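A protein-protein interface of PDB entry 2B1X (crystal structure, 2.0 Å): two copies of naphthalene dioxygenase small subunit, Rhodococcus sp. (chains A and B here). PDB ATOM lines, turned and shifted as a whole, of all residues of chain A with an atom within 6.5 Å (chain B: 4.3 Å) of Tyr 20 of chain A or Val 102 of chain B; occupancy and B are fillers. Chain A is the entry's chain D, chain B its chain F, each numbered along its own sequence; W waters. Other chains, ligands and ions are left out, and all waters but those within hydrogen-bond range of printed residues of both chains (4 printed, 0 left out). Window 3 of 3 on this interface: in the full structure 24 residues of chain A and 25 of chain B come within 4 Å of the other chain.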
ATOM      1  N   ILE A  15     -34.429  -2.956  10.700  1.00  0.00           N
ATOM      2  CA  ILE A  15     -33.425  -3.593   9.852  1.00  0.00           C
ATOM      3  C   ILE A  15     -32.758  -2.585   8.923  1.00  0.00           C
ATOM      4  O   ILE A  15     -31.545  -2.580   8.820  1.00  0.00           O
ATOM      5  CB  ILE A  15     -33.997  -4.819   9.100  1.00  0.00           C
ATOM      6  CG1 ILE A  15     -34.167  -5.978  10.088  1.00  0.00           C
ATOM      7  CG2 ILE A  15     -33.087  -5.260   7.948  1.00  0.00           C
ATOM      8  CD1 ILE A  15     -34.972  -7.149   9.550  1.00  0.00           C
ATOM      9  N   THR A  16     -33.553  -1.733   8.289  1.00  0.00           N
ATOM     10  CA  THR A  16     -33.030  -0.705   7.396  1.00  0.00           C
ATOM     11  C   THR A  16     -32.080   0.241   8.144  1.00  0.00           C
ATOM     12  O   THR A  16     -30.950   0.475   7.688  1.00  0.00           O
ATOM     13  CB  THR A  16     -34.173   0.053   6.668  1.00  0.00           C
ATOM     14  OG1 THR A  16     -34.931  -0.879   5.865  1.00  0.00           O
ATOM     15  CG2 THR A  16     -33.612   1.021   5.632  1.00  0.00           C
ATOM     16  N   GLU A  17     -32.514   0.726   9.307  1.00  0.00           N
ATOM     17  CA  GLU A  17     -31.670   1.582  10.144  1.00  0.00           C
ATOM     18  C   GLU A  17     -30.394   0.843  10.560  1.00  0.00           C
ATOM     19  O   GLU A  17     -29.319   1.409  10.511  1.00  0.00           O
ATOM     20  CB  GLU A  17     -32.459   2.151  11.347  1.00  0.00           C
ATOM     21  CG  GLU A  17     -33.427   3.250  10.913  1.00  0.00           C
ATOM     22  CD  GLU A  17     -34.209   3.951  12.034  1.00  0.00           C
ATOM     23  OE1 GLU A  17     -34.388   3.410  13.165  1.00  0.00           O
ATOM     24  OE2 GLU A  17     -34.675   5.077  11.754  1.00  0.00           O
ATOM     25  N   TRP A  18     -30.524  -0.441  10.903  1.00  0.00           N
ATOM     26  CA  TRP A  18     -29.373  -1.298  11.203  1.00  0.00           C
ATOM     27  C   TRP A  18     -28.362  -1.344  10.033  1.00  0.00           C
ATOM     28  O   TRP A  18     -27.164  -1.223  10.257  1.00  0.00           O
ATOM     29  CB  TRP A  18     -29.828  -2.710  11.616  1.00  0.00           C
ATOM     30  CG  TRP A  18     -28.725  -3.551  12.198  1.00  0.00           C
ATOM     31  CD1 TRP A  18     -28.444  -3.753  13.548  1.00  0.00           C
ATOM     32  CD2 TRP A  18     -27.746  -4.314  11.474  1.00  0.00           C
ATOM     33  NE1 TRP A  18     -27.365  -4.596  13.673  1.00  0.00           N
ATOM     34  CE2 TRP A  18     -26.915  -4.952  12.430  1.00  0.00           C
ATOM     35  CE3 TRP A  18     -27.480  -4.524  10.112  1.00  0.00           C
ATOM     36  CZ2 TRP A  18     -25.851  -5.780  12.063  1.00  0.00           C
ATOM     37  CZ3 TRP A  18     -26.409  -5.342   9.752  1.00  0.00           C
ATOM     38  CH2 TRP A  18     -25.608  -5.953  10.725  1.00  0.00           C
ATOM     39  N   LEU A  19     -28.848  -1.506   8.801  1.00  0.00           N
ATOM     40  CA  LEU A  19     -27.967  -1.478   7.619  1.00  0.00           C
ATOM     41  C   LEU A  19     -27.246  -0.126   7.470  1.00  0.00           C
ATOM     42  O   LEU A  19     -26.041  -0.070   7.117  1.00  0.00           O
ATOM     43  CB  LEU A  19     -28.755  -1.816   6.334  1.00  0.00           C
ATOM     44  CG  LEU A  19     -29.214  -3.274   6.168  1.00  0.00           C
ATOM     45  CD1 LEU A  19     -30.132  -3.442   4.924  1.00  0.00           C
ATOM     46  CD2 LEU A  19     -28.009  -4.232   6.094  1.00  0.00           C
ATOM     47  N   TYR A  20     -27.962   0.959   7.747  1.00  0.00           N
ATOM     48  CA  TYR A  20     -27.365   2.269   7.533  1.00  0.00           C
ATOM     49  C   TYR A  20     -26.317   2.563   8.595  1.00  0.00           C
ATOM     50  O   TYR A  20     -25.263   3.115   8.274  1.00  0.00           O
ATOM     51  CB  TYR A  20     -28.420   3.379   7.449  1.00  0.00           C
ATOM     52  CG  TYR A  20     -29.401   3.264   6.282  1.00  0.00           C
ATOM     53  CD1 TYR A  20     -30.597   3.988   6.312  1.00  0.00           C
ATOM     54  CD2 TYR A  20     -29.118   2.485   5.132  1.00  0.00           C
ATOM     55  CE1 TYR A  20     -31.518   3.930   5.271  1.00  0.00           C
ATOM     56  CE2 TYR A  20     -30.076   2.380   4.067  1.00  0.00           C
ATOM     57  CZ  TYR A  20     -31.264   3.140   4.150  1.00  0.00           C
ATOM     58  OH  TYR A  20     -32.221   3.124   3.149  1.00  0.00           O
ATOM     59  N   MET A  21     -26.592   2.130   9.833  1.00  0.00           N
ATOM     60  CA  MET A  21     -25.646   2.220  10.935  1.00  0.00           C
ATOM     61  C   MET A  21     -24.389   1.406  10.662  1.00  0.00           C
ATOM     62  O   MET A  21     -23.268   1.884  10.905  1.00  0.00           O
ATOM     63  CB  MET A  21     -26.320   1.774  12.238  1.00  0.00           C
ATOM     64  CG  MET A  21     -25.405   1.600  13.433  1.00  0.00           C
ATOM     65  SD  MET A  21     -24.466   0.074  13.486  1.00  0.00           S
ATOM     66  CE  MET A  21     -25.842  -1.214  13.568  1.00  0.00           C
ATOM     67  N   GLU A  22     -24.575   0.177  10.185  1.00  0.00           N
ATOM     68  CA  GLU A  22     -23.454  -0.673   9.777  1.00  0.00           C
ATOM     69  C   GLU A  22     -22.565   0.019   8.749  1.00  0.00           C
ATOM     70  O   GLU A  22     -21.351   0.033   8.874  1.00  0.00           O
ATOM     71  CB  GLU A  22     -23.962  -1.995   9.188  1.00  0.00           C
ATOM     72  CG  GLU A  22     -22.885  -3.052   9.034  1.00  0.00           C
ATOM     73  CD  GLU A  22     -23.055  -3.966   7.821  1.00  0.00           C
ATOM     74  OE1 GLU A  22     -24.102  -3.901   7.134  1.00  0.00           O
ATOM     75  OE2 GLU A  22     -22.126  -4.782   7.575  1.00  0.00           O
ATOM     76  N   ALA A  23     -23.190   0.551   7.711  1.00  0.00           N
ATOM     77  CA  ALA A  23     -22.475   1.166   6.596  1.00  0.00           C
ATOM     78  C   ALA A  23     -21.701   2.399   7.106  1.00  0.00           C
ATOM     79  O   ALA A  23     -20.510   2.616   6.766  1.00  0.00           O
ATOM     80  CB  ALA A  23     -23.476   1.529   5.447  1.00  0.00           C
ATOM     81  N   GLU A  24     -22.368   3.164   7.960  1.00  0.00           N
ATOM     82  CA  GLU A  24     -21.746   4.308   8.647  1.00  0.00           C
ATOM     83  C   GLU A  24     -20.490   3.925   9.422  1.00  0.00           C
ATOM     84  O   GLU A  24     -19.488   4.609   9.293  1.00  0.00           O
ATOM     85  CB  GLU A  24     -22.731   5.003   9.568  1.00  0.00           C
ATOM     86  CG  GLU A  24     -22.220   6.294  10.173  1.00  0.00           C
ATOM     87  CD  GLU A  24     -23.134   6.857  11.238  1.00  0.00           C
ATOM     88  OE1 GLU A  24     -24.298   7.249  10.935  1.00  0.00           O
ATOM     89  OE2 GLU A  24     -22.681   6.916  12.405  1.00  0.00           O
ATOM     90  N   LEU A  25     -20.544   2.848  10.220  1.00  0.00           N
ATOM     91  CA  LEU A  25     -19.346   2.384  10.924  1.00  0.00           C
ATOM     92  C   LEU A  25     -18.215   2.075   9.952  1.00  0.00           C
ATOM     93  O   LEU A  25     -17.076   2.514  10.145  1.00  0.00           O
ATOM     94  CB  LEU A  25     -19.607   1.147  11.793  1.00  0.00           C
ATOM     95  CG  LEU A  25     -20.500   1.277  13.039  1.00  0.00           C
ATOM     96  CD1 LEU A  25     -20.551  -0.065  13.774  1.00  0.00           C
ATOM     97  CD2 LEU A  25     -20.051   2.400  14.001  1.00  0.00           C
ATOM     98  N   VAL A  99     -26.280   1.971   0.078  1.00  0.00           N
ATOM     99  CA  VAL A  99     -27.093   0.790   0.321  1.00  0.00           C
ATOM    100  C   VAL A  99     -28.535   1.117  -0.112  1.00  0.00           C
ATOM    101  O   VAL A  99     -29.155   2.015   0.466  1.00  0.00           O
ATOM    102  CB  VAL A  99     -27.012   0.407   1.814  1.00  0.00           C
ATOM    103  CG1 VAL A  99     -27.947  -0.765   2.152  1.00  0.00           C
ATOM    104  CG2 VAL A  99     -25.511   0.141   2.212  1.00  0.00           C
ATOM    105  N   THR A 100     -29.035   0.441  -1.159  1.00  0.00           N
ATOM    106  CA  THR A 100     -30.320   0.781  -1.763  1.00  0.00           C
ATOM    107  C   THR A 100     -31.102  -0.499  -1.988  1.00  0.00           C
ATOM    108  O   THR A 100     -30.592  -1.596  -1.711  1.00  0.00           O
ATOM    109  CB  THR A 100     -30.159   1.530  -3.122  1.00  0.00           C
ATOM    110  OG1 THR A 100     -29.690   0.610  -4.123  1.00  0.00           O
ATOM    111  CG2 THR A 100     -29.078   2.613  -3.087  1.00  0.00           C
ATOM    112  N   VAL A 102     -33.421  -2.052  -0.484  1.00  0.00           N
ATOM    113  CA  VAL A 102     -33.429  -2.969   0.645  1.00  0.00           C
ATOM    114  C   VAL A 102     -34.699  -3.851   0.637  1.00  0.00           C
ATOM    115  O   VAL A 102     -35.807  -3.321   0.592  1.00  0.00           O
ATOM    116  CB  VAL A 102     -33.306  -2.228   1.968  1.00  0.00           C
ATOM    117  CG1 VAL A 102     -33.456  -3.228   3.163  1.00  0.00           C
ATOM    118  CG2 VAL A 102     -31.974  -1.453   2.006  1.00  0.00           C
ATOM    119  N   THR B  16     -37.721  12.372   4.963  1.00  0.00           N
ATOM    120  CA  THR B  16     -37.220  11.662   3.789  1.00  0.00           C
ATOM    121  C   THR B  16     -37.833  12.243   2.523  1.00  0.00           C
ATOM    122  O   THR B  16     -37.096  12.547   1.581  1.00  0.00           O
ATOM    123  CB  THR B  16     -37.447  10.139   3.901  1.00  0.00           C
ATOM    124  OG1 THR B  16     -36.688   9.630   5.004  1.00  0.00           O
ATOM    125  CG2 THR B  16     -36.802   9.392   2.721  1.00  0.00           C
ATOM    126  N   LEU B  19     -36.279  15.550   1.691  1.00  0.00           N
ATOM    127  CA  LEU B  19     -34.962  15.414   1.049  1.00  0.00           C
ATOM    128  C   LEU B  19     -35.068  15.085  -0.436  1.00  0.00           C
ATOM    129  O   LEU B  19     -34.254  15.538  -1.265  1.00  0.00           O
ATOM    130  CB  LEU B  19     -34.119  14.324   1.749  1.00  0.00           C
ATOM    131  CG  LEU B  19     -33.548  14.633   3.154  1.00  0.00           C
ATOM    132  CD1 LEU B  19     -32.937  13.383   3.762  1.00  0.00           C
ATOM    133  CD2 LEU B  19     -32.520  15.739   3.079  1.00  0.00           C
ATOM    134  N   VAL B  99     -29.791  10.271  -3.302  1.00  0.00           N
ATOM    135  CA  VAL B  99     -29.822  10.462  -1.858  1.00  0.00           C
ATOM    136  C   VAL B  99     -30.229   9.140  -1.217  1.00  0.00           C
ATOM    137  O   VAL B  99     -31.369   8.628  -1.467  1.00  0.00           O
ATOM    138  CB  VAL B  99     -30.846  11.571  -1.483  1.00  0.00           C
ATOM    139  CG1 VAL B  99     -30.979  11.742   0.034  1.00  0.00           C
ATOM    140  CG2 VAL B  99     -30.489  12.933  -2.186  1.00  0.00           C
ATOM    141  N   THR B 100     -29.303   8.542  -0.460  1.00  0.00           N
ATOM    142  CA  THR B 100     -29.513   7.210   0.148  1.00  0.00           C
ATOM    143  C   THR B 100     -29.089   7.211   1.616  1.00  0.00           C
ATOM    144  O   THR B 100     -28.600   8.228   2.118  1.00  0.00           O
ATOM    145  CB  THR B 100     -28.704   6.102  -0.574  1.00  0.00           C
ATOM    146  OG1 THR B 100     -27.328   6.230  -0.227  1.00  0.00           O
ATOM    147  CG2 THR B 100     -28.734   6.208  -2.145  1.00  0.00           C
ATOM    148  N   ASN B 101     -29.225   6.057   2.271  1.00  0.00           N
ATOM    149  CA  ASN B 101     -28.756   5.830   3.631  1.00  0.00           C
ATOM    150  C   ASN B 101     -29.217   6.962   4.543  1.00  0.00           C
ATOM    151  O   ASN B 101     -28.413   7.533   5.304  1.00  0.00           O
ATOM    152  CB  ASN B 101     -27.215   5.720   3.717  1.00  0.00           C
ATOM    153  CG  ASN B 101     -26.639   4.554   2.920  1.00  0.00           C
ATOM    154  OD1 ASN B 101     -25.888   3.731   3.468  1.00  0.00           O
ATOM    155  ND2 ASN B 101     -26.963   4.477   1.639  1.00  0.00           N
ATOM    156  N   VAL B 102     -30.499   7.310   4.463  1.00  0.00           N
ATOM    157  CA  VAL B 102     -30.997   8.432   5.237  1.00  0.00           C
ATOM    158  C   VAL B 102     -31.145   8.048   6.699  1.00  0.00           C
ATOM    159  O   VAL B 102     -31.853   7.077   7.011  1.00  0.00           O
ATOM    160  CB  VAL B 102     -32.309   8.982   4.695  1.00  0.00           C
ATOM    161  CG1 VAL B 102     -32.842  10.110   5.622  1.00  0.00           C
ATOM    162  CG2 VAL B 102     -32.115   9.501   3.227  1.00  0.00           C
ATOM    163  N   ARG B 103     -30.479   8.816   7.573  1.00  0.00           N
ATOM    164  CA  ARG B 103     -30.555   8.630   9.025  1.00  0.00           C
ATOM    165  C   ARG B 103     -31.126   9.905   9.649  1.00  0.00           C
ATOM    166  O   ARG B 103     -30.679  11.003   9.348  1.00  0.00           O
ATOM    167  CB  ARG B 103     -29.176   8.317   9.633  1.00  0.00           C
ATOM    168  CG  ARG B 103     -28.584   6.935   9.246  1.00  0.00           C
ATOM    169  CD  ARG B 103     -27.091   6.982   8.983  1.00  0.00           C
ATOM    170  NE  ARG B 103     -26.852   7.518   7.643  1.00  0.00           N
ATOM    171  CZ  ARG B 103     -25.695   7.960   7.195  1.00  0.00           C
ATOM    172  NH1 ARG B 103     -24.621   7.941   7.996  1.00  0.00           N
ATOM    173  NH2 ARG B 103     -25.612   8.386   5.931  1.00  0.00           N
ATOM    174  N   VAL B 104     -32.134   9.749  10.499  1.00  0.00           N
ATOM    175  CA  VAL B 104     -32.740  10.884  11.204  1.00  0.00           C
ATOM    176  C   VAL B 104     -32.592  10.731  12.718  1.00  0.00           C
ATOM    177  O   VAL B 104     -32.893   9.661  13.273  1.00  0.00           O
ATOM    178  CB  VAL B 104     -34.214  11.039  10.825  1.00  0.00           C
ATOM    179  CG1 VAL B 104     -34.835  12.287  11.506  1.00  0.00           C
ATOM    180  CG2 VAL B 104     -34.374  11.111   9.325  1.00  0.00           C
ATOM    181  N   THR B 116     -28.711  12.865   8.262  1.00  0.00           N
ATOM    182  CA  THR B 116     -27.509  12.413   7.575  1.00  0.00           C
ATOM    183  C   THR B 116     -27.910  11.526   6.414  1.00  0.00           C
ATOM    184  O   THR B 116     -28.726  10.592   6.566  1.00  0.00           O
ATOM    185  CB  THR B 116     -26.597  11.653   8.561  1.00  0.00           C
ATOM    186  OG1 THR B 116     -26.492  12.421   9.774  1.00  0.00           O
ATOM    187  CG2 THR B 116     -25.188  11.603   8.069  1.00  0.00           C
ATOM    188  N   SER B 117     -27.349  11.820   5.250  1.00  0.00           N
ATOM    189  CA  SER B 117     -27.656  11.067   4.034  1.00  0.00           C
ATOM    190  C   SER B 117     -26.416  10.902   3.179  1.00  0.00           C
ATOM    191  O   SER B 117     -25.520  11.722   3.231  1.00  0.00           O
ATOM    192  CB  SER B 117     -28.807  11.735   3.250  1.00  0.00           C
ATOM    193  OG  SER B 117     -28.561  13.124   2.956  1.00  0.00           O
HETATM  194  O   HOH W   1     -30.847   4.026   1.006  1.00  0.00           O
HETATM  195  O   HOH W   2     -25.114   4.716   6.123  1.00  0.00           O
HETATM  196  O   HOH W   3     -34.059   7.275  10.351  1.00  0.00           O
HETATM  197  O   HOH W   4     -32.471   6.204   2.685  1.00  0.00           O
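OE1 of Glu 24 of chain A is in salt-bridge range of NH1 of Arg 103 of chain B.
The side-chain amide nitrogen (ND2) of Asn 101 of chain B sits close to the backbone NH (N) of Val 99 of chain A (3.0 Å).
The side-chain hydroxyl of Thr 100 of chain B is in hydrogen-bond range of the side-chain amide nitrogen of Asn 101 of chain B, 2.6 Å away.
The guanidinium group of Arg 103 of chain B is in hydrogen-bond range of the backbone carbonyl oxygen of Asn 101 of chain B (2.8 Å).
The backbone NH (N) of Arg 103 of chain B sits at hydrogen-bond distance from the backbone carbonyl oxygen (O) of Thr 116 of chain B, 2.7 Å away.
Asn 101 of chain B touches Tyr 20 of chain A.
Tyr 20 of chain A touches Val 102 of chain B.
CB of Tyr 20 of chain A touches CG of Arg 103 of chain B, 3.99 Å away.
CB of Ala 23 of chain A touches OD1 of Asn 101 of chain B, at 3.8 Å.
Thr 100 of chain A touches Thr 100 of chain B.
Of the printed residues of chain B, Tyr 20 of chain A touches Asn 101 (3.7 Å), Val 102 (3.4 Å) and Arg 103 (3.99 Å).
Of chain A, only Tyr 20 comes within 4 Å of Val 102 of chain B.
Of the printed residues of chain A, Asn 101 of chain B touches Tyr 20 (3.7 Å), Ala 23 (3.8 Å) and Val 99 (3.0 Å).
Of the printed residues of chain B, Val 99 of chain A touches Asn 101.
Of the printed residues of chain B, Ala 23 of chain A touches Asn 101 (3.8 Å).
Leu 19 of chain B touches none of the printed residues of chain A.
Trp 18 of chain A touches none of the printed residues of chain B.
The nearest printed residue of chain A that does not touch Arg 103 of chain B is Met 21 of chain A (5.0 Å).
Printed residues of chain A that touch a printed residue of chain B: Tyr 20, Ala 23, Glu 24, Val 99 and Thr 100.
Hydrophobic or aromatic side chains of chain A that line the printed part of chain B: Tyr 20, Ala 23 and Val 99.
Printed residues of chain B that touch a printed residue of chain A: Thr 100, Asn 101, Val 102 and Arg 103.
Along chain B the printed residues that touch a printed residue of chain A span positions 100 to 103.
Among the printed residues, 7 pairs touch across the chains.
Among the printed residues, Asp or Glu carboxylates within 4 Å of a Lys or Arg side-chain nitrogen of the other chain: Glu 24 of chain A with Arg 103 of chain B.
Thr 100 of chain A touches its own counterpart, Thr 100 of chain B.
Of the 7 pairs that touch across the chains among the printed residues, 1 has its exchanged pair printed and touching as well.
Water W3 lies within hydrogen-bond range of the side-chain carboxylate (OE2) of Glu 17 of chain A and the backbone NH (N) of Val 104 of chain B.
Water W1 lies within hydrogen-bond range of O of Val 99 of chain A (2.7 Å), OH of Tyr 20 of chain A (2.7 Å) and N of Asn 101 of chain B (2.9 Å).
Water W2 lies within hydrogen-bond range of O of Tyr 20 of chain A (2.7 Å) and OD1 of Asn 101 of chain B (2.9 Å).
Water W4 lies within hydrogen-bond range of N of Val 102 of chain B (2.9 Å), OH of Tyr 20 of chain A (3.1 Å) and N of Asn 101 of chain B (3.3 Å).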
